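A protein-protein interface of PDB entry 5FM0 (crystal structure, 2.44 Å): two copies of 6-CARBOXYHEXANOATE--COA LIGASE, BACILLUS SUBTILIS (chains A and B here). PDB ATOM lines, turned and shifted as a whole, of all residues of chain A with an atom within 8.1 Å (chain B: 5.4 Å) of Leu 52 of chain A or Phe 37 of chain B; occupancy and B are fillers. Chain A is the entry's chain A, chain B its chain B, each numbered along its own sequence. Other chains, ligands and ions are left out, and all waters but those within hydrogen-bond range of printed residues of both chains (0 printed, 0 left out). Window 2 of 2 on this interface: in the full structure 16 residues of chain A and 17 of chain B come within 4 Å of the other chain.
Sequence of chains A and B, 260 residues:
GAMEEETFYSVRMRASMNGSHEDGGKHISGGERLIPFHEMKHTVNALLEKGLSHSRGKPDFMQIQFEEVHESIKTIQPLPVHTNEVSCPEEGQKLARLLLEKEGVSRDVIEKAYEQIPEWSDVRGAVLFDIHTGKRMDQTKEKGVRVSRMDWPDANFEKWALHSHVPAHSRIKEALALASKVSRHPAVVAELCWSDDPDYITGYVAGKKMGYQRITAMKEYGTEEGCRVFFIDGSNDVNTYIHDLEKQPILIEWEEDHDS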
ATOM      1  N   MET A  13      13.852  16.499 -23.362  1.00  0.00           N
ATOM      2  CA  MET A  13      13.207  15.268 -22.969  1.00  0.00           C
ATOM      3  C   MET A  13      13.446  15.022 -21.495  1.00  0.00           C
ATOM      4  O   MET A  13      14.519  15.313 -20.975  1.00  0.00           O
ATOM      5  CB  MET A  13      13.772  14.111 -23.786  1.00  0.00           C
ATOM      6  CG  MET A  13      13.163  12.755 -23.467  1.00  0.00           C
ATOM      7  SD  MET A  13      13.910  11.995 -22.014  1.00  0.00           S
ATOM      8  CE  MET A  13      15.547  11.584 -22.632  1.00  0.00           C
ATOM      9  N   ALA A  15      12.314  11.708 -18.522  1.00  0.00           N
ATOM     10  CA  ALA A  15      11.665  10.445 -18.316  1.00  0.00           C
ATOM     11  C   ALA A  15      11.833  10.023 -16.852  1.00  0.00           C
ATOM     12  O   ALA A  15      12.850  10.289 -16.240  1.00  0.00           O
ATOM     13  CB  ALA A  15      12.252   9.412 -19.247  1.00  0.00           C
ATOM     14  N   ILE A  28      14.861   8.985 -14.528  1.00  0.00           N
ATOM     15  CA  ILE A  28      15.528   7.975 -15.341  1.00  0.00           C
ATOM     16  C   ILE A  28      16.502   8.657 -16.298  1.00  0.00           C
ATOM     17  O   ILE A  28      17.665   8.299 -16.358  1.00  0.00           O
ATOM     18  CB  ILE A  28      14.506   7.155 -16.168  1.00  0.00           C
ATOM     19  CG1 ILE A  28      13.624   6.307 -15.245  1.00  0.00           C
ATOM     20  CG2 ILE A  28      15.199   6.266 -17.192  1.00  0.00           C
ATOM     21  CD1 ILE A  28      14.374   5.212 -14.522  1.00  0.00           C
ATOM     22  N   SER A  29      16.010   9.649 -17.041  1.00  0.00           N
ATOM     23  CA  SER A  29      16.783  10.251 -18.111  1.00  0.00           C
ATOM     24  C   SER A  29      16.312  11.658 -18.445  1.00  0.00           C
ATOM     25  O   SER A  29      15.212  12.069 -18.110  1.00  0.00           O
ATOM     26  CB  SER A  29      16.718   9.380 -19.375  1.00  0.00           C
ATOM     27  OG  SER A  29      17.497   9.935 -20.424  1.00  0.00           O
ATOM     28  N   ASN A  45      13.305  11.280 -32.323  1.00  0.00           N
ATOM     29  CA  ASN A  45      13.572   9.848 -32.233  1.00  0.00           C
ATOM     30  C   ASN A  45      14.798   9.492 -31.406  1.00  0.00           C
ATOM     31  O   ASN A  45      14.780   8.508 -30.650  1.00  0.00           O
ATOM     32  CB  ASN A  45      13.664   9.269 -33.623  1.00  0.00           C
ATOM     33  CG  ASN A  45      12.285   9.006 -34.209  1.00  0.00           C
ATOM     34  OD1 ASN A  45      11.565   8.140 -33.725  1.00  0.00           O
ATOM     35  ND2 ASN A  45      11.896   9.766 -35.219  1.00  0.00           N
ATOM     36  N   ALA A  46      15.855  10.292 -31.515  1.00  0.00           N
ATOM     37  CA  ALA A  46      17.059  10.001 -30.740  1.00  0.00           C
ATOM     38  C   ALA A  46      16.750  10.138 -29.260  1.00  0.00           C
ATOM     39  O   ALA A  46      17.135   9.296 -28.442  1.00  0.00           O
ATOM     40  CB  ALA A  46      18.207  10.933 -31.138  1.00  0.00           C
ATOM     41  N   LEU A  47      16.044  11.200 -28.912  1.00  0.00           N
ATOM     42  CA  LEU A  47      15.732  11.436 -27.516  1.00  0.00           C
ATOM     43  C   LEU A  47      14.795  10.376 -26.986  1.00  0.00           C
ATOM     44  O   LEU A  47      14.891   9.964 -25.826  1.00  0.00           O
ATOM     45  CB  LEU A  47      15.101  12.814 -27.329  1.00  0.00           C
ATOM     46  CG  LEU A  47      16.077  13.963 -27.483  1.00  0.00           C
ATOM     47  CD1 LEU A  47      15.309  15.268 -27.649  1.00  0.00           C
ATOM     48  CD2 LEU A  47      17.039  14.029 -26.307  1.00  0.00           C
ATOM     49  N   LEU A  48      13.850   9.975 -27.820  1.00  0.00           N
ATOM     50  CA  LEU A  48      12.936   8.915 -27.453  1.00  0.00           C
ATOM     51  C   LEU A  48      13.733   7.650 -27.125  1.00  0.00           C
ATOM     52  O   LEU A  48      13.600   7.072 -26.058  1.00  0.00           O
ATOM     53  CB  LEU A  48      11.990   8.645 -28.608  1.00  0.00           C
ATOM     54  CG  LEU A  48      10.957   7.564 -28.347  1.00  0.00           C
ATOM     55  CD1 LEU A  48      10.191   7.808 -27.044  1.00  0.00           C
ATOM     56  CD2 LEU A  48      10.025   7.502 -29.536  1.00  0.00           C
ATOM     57  N   GLU A  49      14.586   7.255 -28.049  1.00  0.00           N
ATOM     58  CA  GLU A  49      15.362   6.039 -27.897  1.00  0.00           C
ATOM     59  C   GLU A  49      16.212   6.092 -26.637  1.00  0.00           C
ATOM     60  O   GLU A  49      16.343   5.109 -25.896  1.00  0.00           O
ATOM     61  CB  GLU A  49      16.236   5.826 -29.146  1.00  0.00           C
ATOM     62  CG  GLU A  49      17.303   4.755 -28.998  1.00  0.00           C
ATOM     63  CD  GLU A  49      16.720   3.370 -28.768  1.00  0.00           C
ATOM     64  OE1 GLU A  49      15.552   3.276 -28.335  1.00  0.00           O
ATOM     65  OE2 GLU A  49      17.429   2.376 -29.021  1.00  0.00           O
ATOM     66  N   LYS A  50      16.789   7.251 -26.386  1.00  0.00           N
ATOM     67  CA  LYS A  50      17.718   7.411 -25.271  1.00  0.00           C
ATOM     68  C   LYS A  50      17.000   7.222 -23.931  1.00  0.00           C
ATOM     69  O   LYS A  50      17.550   6.616 -22.988  1.00  0.00           O
ATOM     70  CB  LYS A  50      18.385   8.783 -25.381  1.00  0.00           C
ATOM     71  CG  LYS A  50      19.034   9.344 -24.140  1.00  0.00           C
ATOM     72  CD  LYS A  50      19.614  10.712 -24.490  1.00  0.00           C
ATOM     73  CE  LYS A  50      19.931  11.552 -23.258  1.00  0.00           C
ATOM     74  NZ  LYS A  50      21.287  11.244 -22.713  1.00  0.00           N
ATOM     75  N   GLY A  51      15.761   7.712 -23.849  1.00  0.00           N
ATOM     76  CA  GLY A  51      14.941   7.527 -22.641  1.00  0.00           C
ATOM     77  C   GLY A  51      14.460   6.093 -22.438  1.00  0.00           C
ATOM     78  O   GLY A  51      14.353   5.625 -21.304  1.00  0.00           O
ATOM     79  N   LEU A  52      14.162   5.405 -23.538  1.00  0.00           N
ATOM     80  CA  LEU A  52      13.607   4.057 -23.491  1.00  0.00           C
ATOM     81  C   LEU A  52      14.623   3.000 -23.069  1.00  0.00           C
ATOM     82  O   LEU A  52      14.281   2.040 -22.384  1.00  0.00           O
ATOM     83  CB  LEU A  52      12.988   3.679 -24.852  1.00  0.00           C
ATOM     84  CG  LEU A  52      11.674   4.408 -25.165  1.00  0.00           C
ATOM     85  CD1 LEU A  52      11.023   3.867 -26.425  1.00  0.00           C
ATOM     86  CD2 LEU A  52      10.705   4.328 -23.996  1.00  0.00           C
ATOM     87  N   SER A  53      15.869   3.168 -23.480  1.00  0.00           N
ATOM     88  CA  SER A  53      16.874   2.148 -23.234  1.00  0.00           C
ATOM     89  C   SER A  53      17.903   2.610 -22.220  1.00  0.00           C
ATOM     90  O   SER A  53      19.092   2.456 -22.433  1.00  0.00           O
ATOM     91  CB  SER A  53      17.574   1.799 -24.540  1.00  0.00           C
ATOM     92  OG  SER A  53      18.283   2.932 -25.010  1.00  0.00           O
ATOM     93  N   HIS A  54      17.456   3.173 -21.111  1.00  0.00           N
ATOM     94  CA  HIS A  54      18.402   3.676 -20.128  1.00  0.00           C
ATOM     95  C   HIS A  54      18.678   2.622 -19.047  1.00  0.00           C
ATOM     96  O   HIS A  54      17.772   1.884 -18.613  1.00  0.00           O
ATOM     97  CB  HIS A  54      17.873   4.963 -19.498  1.00  0.00           C
ATOM     98  CG  HIS A  54      18.933   5.802 -18.847  1.00  0.00           C
ATOM     99  ND1 HIS A  54      19.279   5.677 -17.519  1.00  0.00           N
ATOM    100  CD2 HIS A  54      19.723   6.779 -19.347  1.00  0.00           C
ATOM    101  CE1 HIS A  54      20.236   6.541 -17.229  1.00  0.00           C
ATOM    102  NE2 HIS A  54      20.519   7.225 -18.320  1.00  0.00           N
ATOM    103  N   SER A  55      19.925   2.582 -18.592  1.00  0.00           N
ATOM    104  CA  SER A  55      20.362   1.605 -17.602  1.00  0.00           C
ATOM    105  C   SER A  55      19.701   1.782 -16.225  1.00  0.00           C
ATOM    106  O   SER A  55      19.785   0.893 -15.390  1.00  0.00           O
ATOM    107  CB  SER A  55      21.899   1.645 -17.449  1.00  0.00           C
ATOM    108  OG  SER A  55      22.342   2.758 -16.679  1.00  0.00           O
ATOM    109  N   ARG A  56      19.054   2.921 -15.986  1.00  0.00           N
ATOM    110  CA  ARG A  56      18.419   3.176 -14.685  1.00  0.00           C
ATOM    111  C   ARG A  56      16.986   2.613 -14.616  1.00  0.00           C
ATOM    112  O   ARG A  56      16.335   2.659 -13.564  1.00  0.00           O
ATOM    113  CB  ARG A  56      18.392   4.666 -14.384  1.00  0.00           C
ATOM    114  CG  ARG A  56      19.718   5.246 -13.958  1.00  0.00           C
ATOM    115  CD  ARG A  56      19.646   6.756 -13.826  1.00  0.00           C
ATOM    116  NE  ARG A  56      18.661   7.197 -12.825  1.00  0.00           N
ATOM    117  CZ  ARG A  56      18.937   7.405 -11.536  1.00  0.00           C
ATOM    118  NH1 ARG A  56      20.160   7.185 -11.065  1.00  0.00           N
ATOM    119  NH2 ARG A  56      17.992   7.831 -10.706  1.00  0.00           N
ATOM    120  N   GLY A  57      16.512   2.080 -15.737  1.00  0.00           N
ATOM    121  CA  GLY A  57      15.207   1.459 -15.786  1.00  0.00           C
ATOM    122  C   GLY A  57      14.420   1.901 -16.999  1.00  0.00           C
ATOM    123  O   GLY A  57      14.832   2.796 -17.745  1.00  0.00           O
ATOM    124  N   LYS A  58      13.285   1.246 -17.199  1.00  0.00           N
ATOM    125  CA  LYS A  58      12.351   1.627 -18.232  1.00  0.00           C
ATOM    126  C   LYS A  58      11.332   2.608 -17.626  1.00  0.00           C
ATOM    127  O   LYS A  58      10.825   2.402 -16.510  1.00  0.00           O
ATOM    128  CB  LYS A  58      11.670   0.399 -18.804  1.00  0.00           C
ATOM    129  CG  LYS A  58      10.568   0.710 -19.796  1.00  0.00           C
ATOM    130  CD  LYS A  58       9.800  -0.547 -20.177  1.00  0.00           C
ATOM    131  CE  LYS A  58       8.302  -0.291 -20.209  1.00  0.00           C
ATOM    132  NZ  LYS A  58       7.542  -1.517 -20.577  1.00  0.00           N
ATOM    133  N   PRO A  59      11.061   3.706 -18.343  1.00  0.00           N
ATOM    134  CA  PRO A  59      10.207   4.738 -17.783  1.00  0.00           C
ATOM    135  C   PRO A  59       8.731   4.467 -18.003  1.00  0.00           C
ATOM    136  O   PRO A  59       8.335   3.852 -19.001  1.00  0.00           O
ATOM    137  CB  PRO A  59      10.629   5.982 -18.559  1.00  0.00           C
ATOM    138  CG  PRO A  59      10.987   5.455 -19.897  1.00  0.00           C
ATOM    139  CD  PRO A  59      11.617   4.105 -19.645  1.00  0.00           C
ATOM    140  N   ASP A  60       7.923   4.951 -17.078  1.00  0.00           N
ATOM    141  CA  ASP A  60       6.493   4.949 -17.273  1.00  0.00           C
ATOM    142  C   ASP A  60       5.953   6.380 -17.482  1.00  0.00           C
ATOM    143  O   ASP A  60       4.750   6.596 -17.513  1.00  0.00           O
ATOM    144  CB  ASP A  60       5.801   4.247 -16.104  1.00  0.00           C
ATOM    145  CG  ASP A  60       6.104   4.880 -14.771  1.00  0.00           C
ATOM    146  OD1 ASP A  60       6.388   6.107 -14.728  1.00  0.00           O
ATOM    147  OD2 ASP A  60       6.036   4.144 -13.755  1.00  0.00           O
ATOM    148  N   PHE A  61       6.860   7.341 -17.610  1.00  0.00           N
ATOM    149  CA  PHE A  61       6.519   8.710 -17.936  1.00  0.00           C
ATOM    150  C   PHE A  61       7.610   9.322 -18.811  1.00  0.00           C
ATOM    151  O   PHE A  61       8.786   9.113 -18.581  1.00  0.00           O
ATOM    152  CB  PHE A  61       6.364   9.538 -16.678  1.00  0.00           C
ATOM    153  CG  PHE A  61       6.103  10.988 -16.949  1.00  0.00           C
ATOM    154  CD1 PHE A  61       4.809  11.448 -17.151  1.00  0.00           C
ATOM    155  CD2 PHE A  61       7.141  11.885 -17.026  1.00  0.00           C
ATOM    156  CE1 PHE A  61       4.568  12.783 -17.414  1.00  0.00           C
ATOM    157  CE2 PHE A  61       6.909  13.225 -17.282  1.00  0.00           C
ATOM    158  CZ  PHE A  61       5.620  13.676 -17.476  1.00  0.00           C
ATOM    159  N   MET A  62       7.212  10.057 -19.833  1.00  0.00           N
ATOM    160  CA  MET A  62       8.152  10.773 -20.651  1.00  0.00           C
ATOM    161  C   MET A  62       7.523  12.012 -21.291  1.00  0.00           C
ATOM    162  O   MET A  62       6.374  11.989 -21.694  1.00  0.00           O
ATOM    163  CB  MET A  62       8.717   9.874 -21.736  1.00  0.00           C
ATOM    164  CG  MET A  62       9.807  10.569 -22.557  1.00  0.00           C
ATOM    165  SD  MET A  62      10.590   9.561 -23.836  1.00  0.00           S
ATOM    166  CE  MET A  62      11.192   8.193 -22.869  1.00  0.00           C
ATOM    167  N   THR B   7       0.797  -3.588 -20.032  1.00  0.00           N
ATOM    168  CA  THR B   7       0.092  -2.392 -19.584  1.00  0.00           C
ATOM    169  C   THR B   7      -0.069  -1.390 -20.722  1.00  0.00           C
ATOM    170  O   THR B   7       0.673  -1.401 -21.712  1.00  0.00           O
ATOM    171  CB  THR B   7       0.851  -1.683 -18.463  1.00  0.00           C
ATOM    172  OG1 THR B   7       2.104  -1.229 -18.973  1.00  0.00           O
ATOM    173  CG2 THR B   7       1.077  -2.636 -17.284  1.00  0.00           C
ATOM    174  N   TYR B   9      -0.552   2.666 -22.216  1.00  0.00           N
ATOM    175  CA  TYR B   9       0.047   3.985 -22.088  1.00  0.00           C
ATOM    176  C   TYR B   9      -0.788   5.060 -22.767  1.00  0.00           C
ATOM    177  O   TYR B   9      -1.188   4.912 -23.915  1.00  0.00           O
ATOM    178  CB  TYR B   9       1.458   3.971 -22.709  1.00  0.00           C
ATOM    179  CG  TYR B   9       2.445   3.219 -21.879  1.00  0.00           C
ATOM    180  CD1 TYR B   9       2.539   1.826 -21.941  1.00  0.00           C
ATOM    181  CD2 TYR B   9       3.265   3.885 -21.007  1.00  0.00           C
ATOM    182  CE1 TYR B   9       3.444   1.134 -21.143  1.00  0.00           C
ATOM    183  CE2 TYR B   9       4.164   3.211 -20.224  1.00  0.00           C
ATOM    184  CZ  TYR B   9       4.253   1.843 -20.292  1.00  0.00           C
ATOM    185  OH  TYR B   9       5.156   1.202 -19.473  1.00  0.00           O
ATOM    186  N   ILE B  35      -2.303   3.043 -25.932  1.00  0.00           N
ATOM    187  CA  ILE B  35      -1.619   2.006 -26.663  1.00  0.00           C
ATOM    188  C   ILE B  35      -0.773   1.119 -25.779  1.00  0.00           C
ATOM    189  O   ILE B  35      -0.390   1.519 -24.676  1.00  0.00           O
ATOM    190  CB  ILE B  35      -0.640   2.615 -27.671  1.00  0.00           C
ATOM    191  CG1 ILE B  35       0.309   3.558 -26.955  1.00  0.00           C
ATOM    192  CG2 ILE B  35      -1.384   3.345 -28.778  1.00  0.00           C
ATOM    193  CD1 ILE B  35       1.623   3.760 -27.659  1.00  0.00           C
ATOM    194  N   PRO B  36      -0.483  -0.102 -26.264  1.00  0.00           N
ATOM    195  CA  PRO B  36       0.492  -0.976 -25.604  1.00  0.00           C
ATOM    196  C   PRO B  36       1.862  -0.425 -25.866  1.00  0.00           C
ATOM    197  O   PRO B  36       2.079   0.284 -26.857  1.00  0.00           O
ATOM    198  CB  PRO B  36       0.290  -2.339 -26.288  1.00  0.00           C
ATOM    199  CG  PRO B  36      -0.313  -2.011 -27.618  1.00  0.00           C
ATOM    200  CD  PRO B  36      -1.054  -0.710 -27.483  1.00  0.00           C
ATOM    201  N   PHE B  37       2.782  -0.729 -24.991  1.00  0.00           N
ATOM    202  CA  PHE B  37       4.086  -0.132 -25.054  1.00  0.00           C
ATOM    203  C   PHE B  37       4.809  -0.316 -26.387  1.00  0.00           C
ATOM    204  O   PHE B  37       5.530   0.590 -26.840  1.00  0.00           O
ATOM    205  CB  PHE B  37       4.945  -0.689 -23.946  1.00  0.00           C
ATOM    206  CG  PHE B  37       6.229   0.045 -23.778  1.00  0.00           C
ATOM    207  CD1 PHE B  37       6.257   1.260 -23.105  1.00  0.00           C
ATOM    208  CD2 PHE B  37       7.410  -0.462 -24.308  1.00  0.00           C
ATOM    209  CE1 PHE B  37       7.446   1.949 -22.947  1.00  0.00           C
ATOM    210  CE2 PHE B  37       8.595   0.216 -24.147  1.00  0.00           C
ATOM    211  CZ  PHE B  37       8.615   1.421 -23.467  1.00  0.00           C
ATOM    212  N   HIS B  38       4.644  -1.481 -27.009  1.00  0.00           N
ATOM    213  CA  HIS B  38       5.410  -1.797 -28.224  1.00  0.00           C
ATOM    214  C   HIS B  38       5.001  -0.963 -29.420  1.00  0.00           C
ATOM    215  O   HIS B  38       5.636  -1.031 -30.468  1.00  0.00           O
ATOM    216  CB  HIS B  38       5.321  -3.292 -28.574  1.00  0.00           C
ATOM    217  CG  HIS B  38       3.932  -3.779 -28.857  1.00  0.00           C
ATOM    218  ND1 HIS B  38       3.307  -3.583 -30.067  1.00  0.00           N
ATOM    219  CD2 HIS B  38       3.056  -4.465 -28.085  1.00  0.00           C
ATOM    220  CE1 HIS B  38       2.093  -4.106 -30.025  1.00  0.00           C
ATOM    221  NE2 HIS B  38       1.921  -4.656 -28.836  1.00  0.00           N
ATOM    222  N   GLU B  39       3.942  -0.175 -29.280  1.00  0.00           N
ATOM    223  CA  GLU B  39       3.557   0.737 -30.340  1.00  0.00           C
ATOM    224  C   GLU B  39       4.025   2.188 -30.060  1.00  0.00           C
ATOM    225  O   GLU B  39       3.602   3.112 -30.737  1.00  0.00           O
ATOM    226  CB  GLU B  39       2.043   0.682 -30.579  1.00  0.00           C
ATOM    227  CG  GLU B  39       1.534  -0.677 -31.034  1.00  0.00           C
ATOM    228  CD  GLU B  39       0.038  -0.699 -31.367  1.00  0.00           C
ATOM    229  OE1 GLU B  39      -0.713   0.175 -30.886  1.00  0.00           O
ATOM    230  OE2 GLU B  39      -0.394  -1.614 -32.109  1.00  0.00           O
ATOM    231  N   MET B  40       4.921   2.362 -29.098  1.00  0.00           N
ATOM    232  CA  MET B  40       5.355   3.667 -28.706  1.00  0.00           C
ATOM    233  C   MET B  40       6.034   4.432 -29.841  1.00  0.00           C
ATOM    234  O   MET B  40       5.676   5.585 -30.116  1.00  0.00           O
ATOM    235  CB  MET B  40       6.254   3.596 -27.486  1.00  0.00           C
ATOM    236  CG  MET B  40       6.431   4.947 -26.813  1.00  0.00           C
ATOM    237  SD  MET B  40       4.864   5.738 -26.310  1.00  0.00           S
ATOM    238  CE  MET B  40       4.574   4.901 -24.757  1.00  0.00           C
ATOM    239  N   LYS B  41       6.998   3.819 -30.512  1.00  0.00           N
ATOM    240  CA  LYS B  41       7.729   4.536 -31.566  1.00  0.00           C
ATOM    241  C   LYS B  41       6.817   5.002 -32.676  1.00  0.00           C
ATOM    242  O   LYS B  41       6.888   6.133 -33.111  1.00  0.00           O
ATOM    243  CB  LYS B  41       8.859   3.682 -32.133  1.00  0.00           C
ATOM    244  CG  LYS B  41       9.674   3.021 -31.036  1.00  0.00           C
ATOM    245  CD  LYS B  41      11.174   3.064 -31.289  1.00  0.00           C
ATOM    246  CE  LYS B  41      11.923   2.389 -30.143  1.00  0.00           C
ATOM    247  NZ  LYS B  41      13.352   2.805 -30.103  1.00  0.00           N
ATOM    248  N   PHE B  66       3.920  10.750 -22.696  1.00  0.00           N
ATOM    249  CA  PHE B  66       3.262   9.498 -22.407  1.00  0.00           C
ATOM    250  C   PHE B  66       3.365   9.161 -20.973  1.00  0.00           C
ATOM    251  O   PHE B  66       4.258   9.633 -20.265  1.00  0.00           O
ATOM    252  CB  PHE B  66       3.761   8.346 -23.299  1.00  0.00           C
ATOM    253  CG  PHE B  66       5.108   7.778 -22.933  1.00  0.00           C
ATOM    254  CD1 PHE B  66       5.275   6.980 -21.815  1.00  0.00           C
ATOM    255  CD2 PHE B  66       6.185   7.956 -23.774  1.00  0.00           C
ATOM    256  CE1 PHE B  66       6.512   6.417 -21.521  1.00  0.00           C
ATOM    257  CE2 PHE B  66       7.419   7.393 -23.488  1.00  0.00           C
ATOM    258  CZ  PHE B  66       7.584   6.621 -22.358  1.00  0.00           C
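Along chain A the printed residues that touch a printed residue of chain B span positions 49 to 62.
Of the 10 printed residues of chain B, 4 touch a printed residue of chain A.
Hydrophobic or aromatic side chains of chain B within 4 Å of the printed part of chain A: Tyr 9, Phe 37 and Phe 66.
O of Glu 49 of chain A is in hydrogen-bond range of OG of Ser 53 of chain A.
N of Tyr 9 of chain B lies within hydrogen-bond range of O of Ile 35 of chain B, 2.7 Å away.
O of Met 62 of chain A lies within hydrogen-bond range of N of Phe 66 of chain B (2.9 Å).
The side-chain amino group of Lys 41 of chain B lies within salt-bridge range of the side-chain carboxylate of Glu 49 of chain A, at 2.9 Å.
Of the printed residues of chain B, Lys 58 of chain A touches Tyr 9 (3.6 Å) and Phe 37 (3.6 Å).
Of the printed residues of chain B, Phe 61 of chain A touches Phe 66 (3.4 Å).
Printed residues of chain B within 4 Å of Met 62 of chain A: Phe 66.
Of the printed residues of chain A, Tyr 9 of chain B touches Lys 58 (3.6 Å).
Pro 36 of chain B touches none of the printed residues of chain A.
Phe 37 of chain B touches two residues of chain A.
Of the printed residues of chain A, Lys 41 of chain B touches Glu 49.
The nearest residue of chain A that does not touch Phe 37 of chain B is Pro 59 of chain A (4.5 Å).
The nearest printed residue of chain B that does not touch Glu 49 of chain A is Phe 66 of chain B (8.5 Å).
No position is printed for both chains.
Of the 6 pairs that touch across the chains among the printed residues, none has its exchanged pair printed and touching as well.
Among the printed residues, merely in contact across the chains: Leu 52 of chain A with Phe 37 of chain B, Lys 58 of chain A with Tyr 9 of chain B, Lys 58 of chain A with Phe 37 of chain B and Phe 61 of chain A with Phe 66 of chain B.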
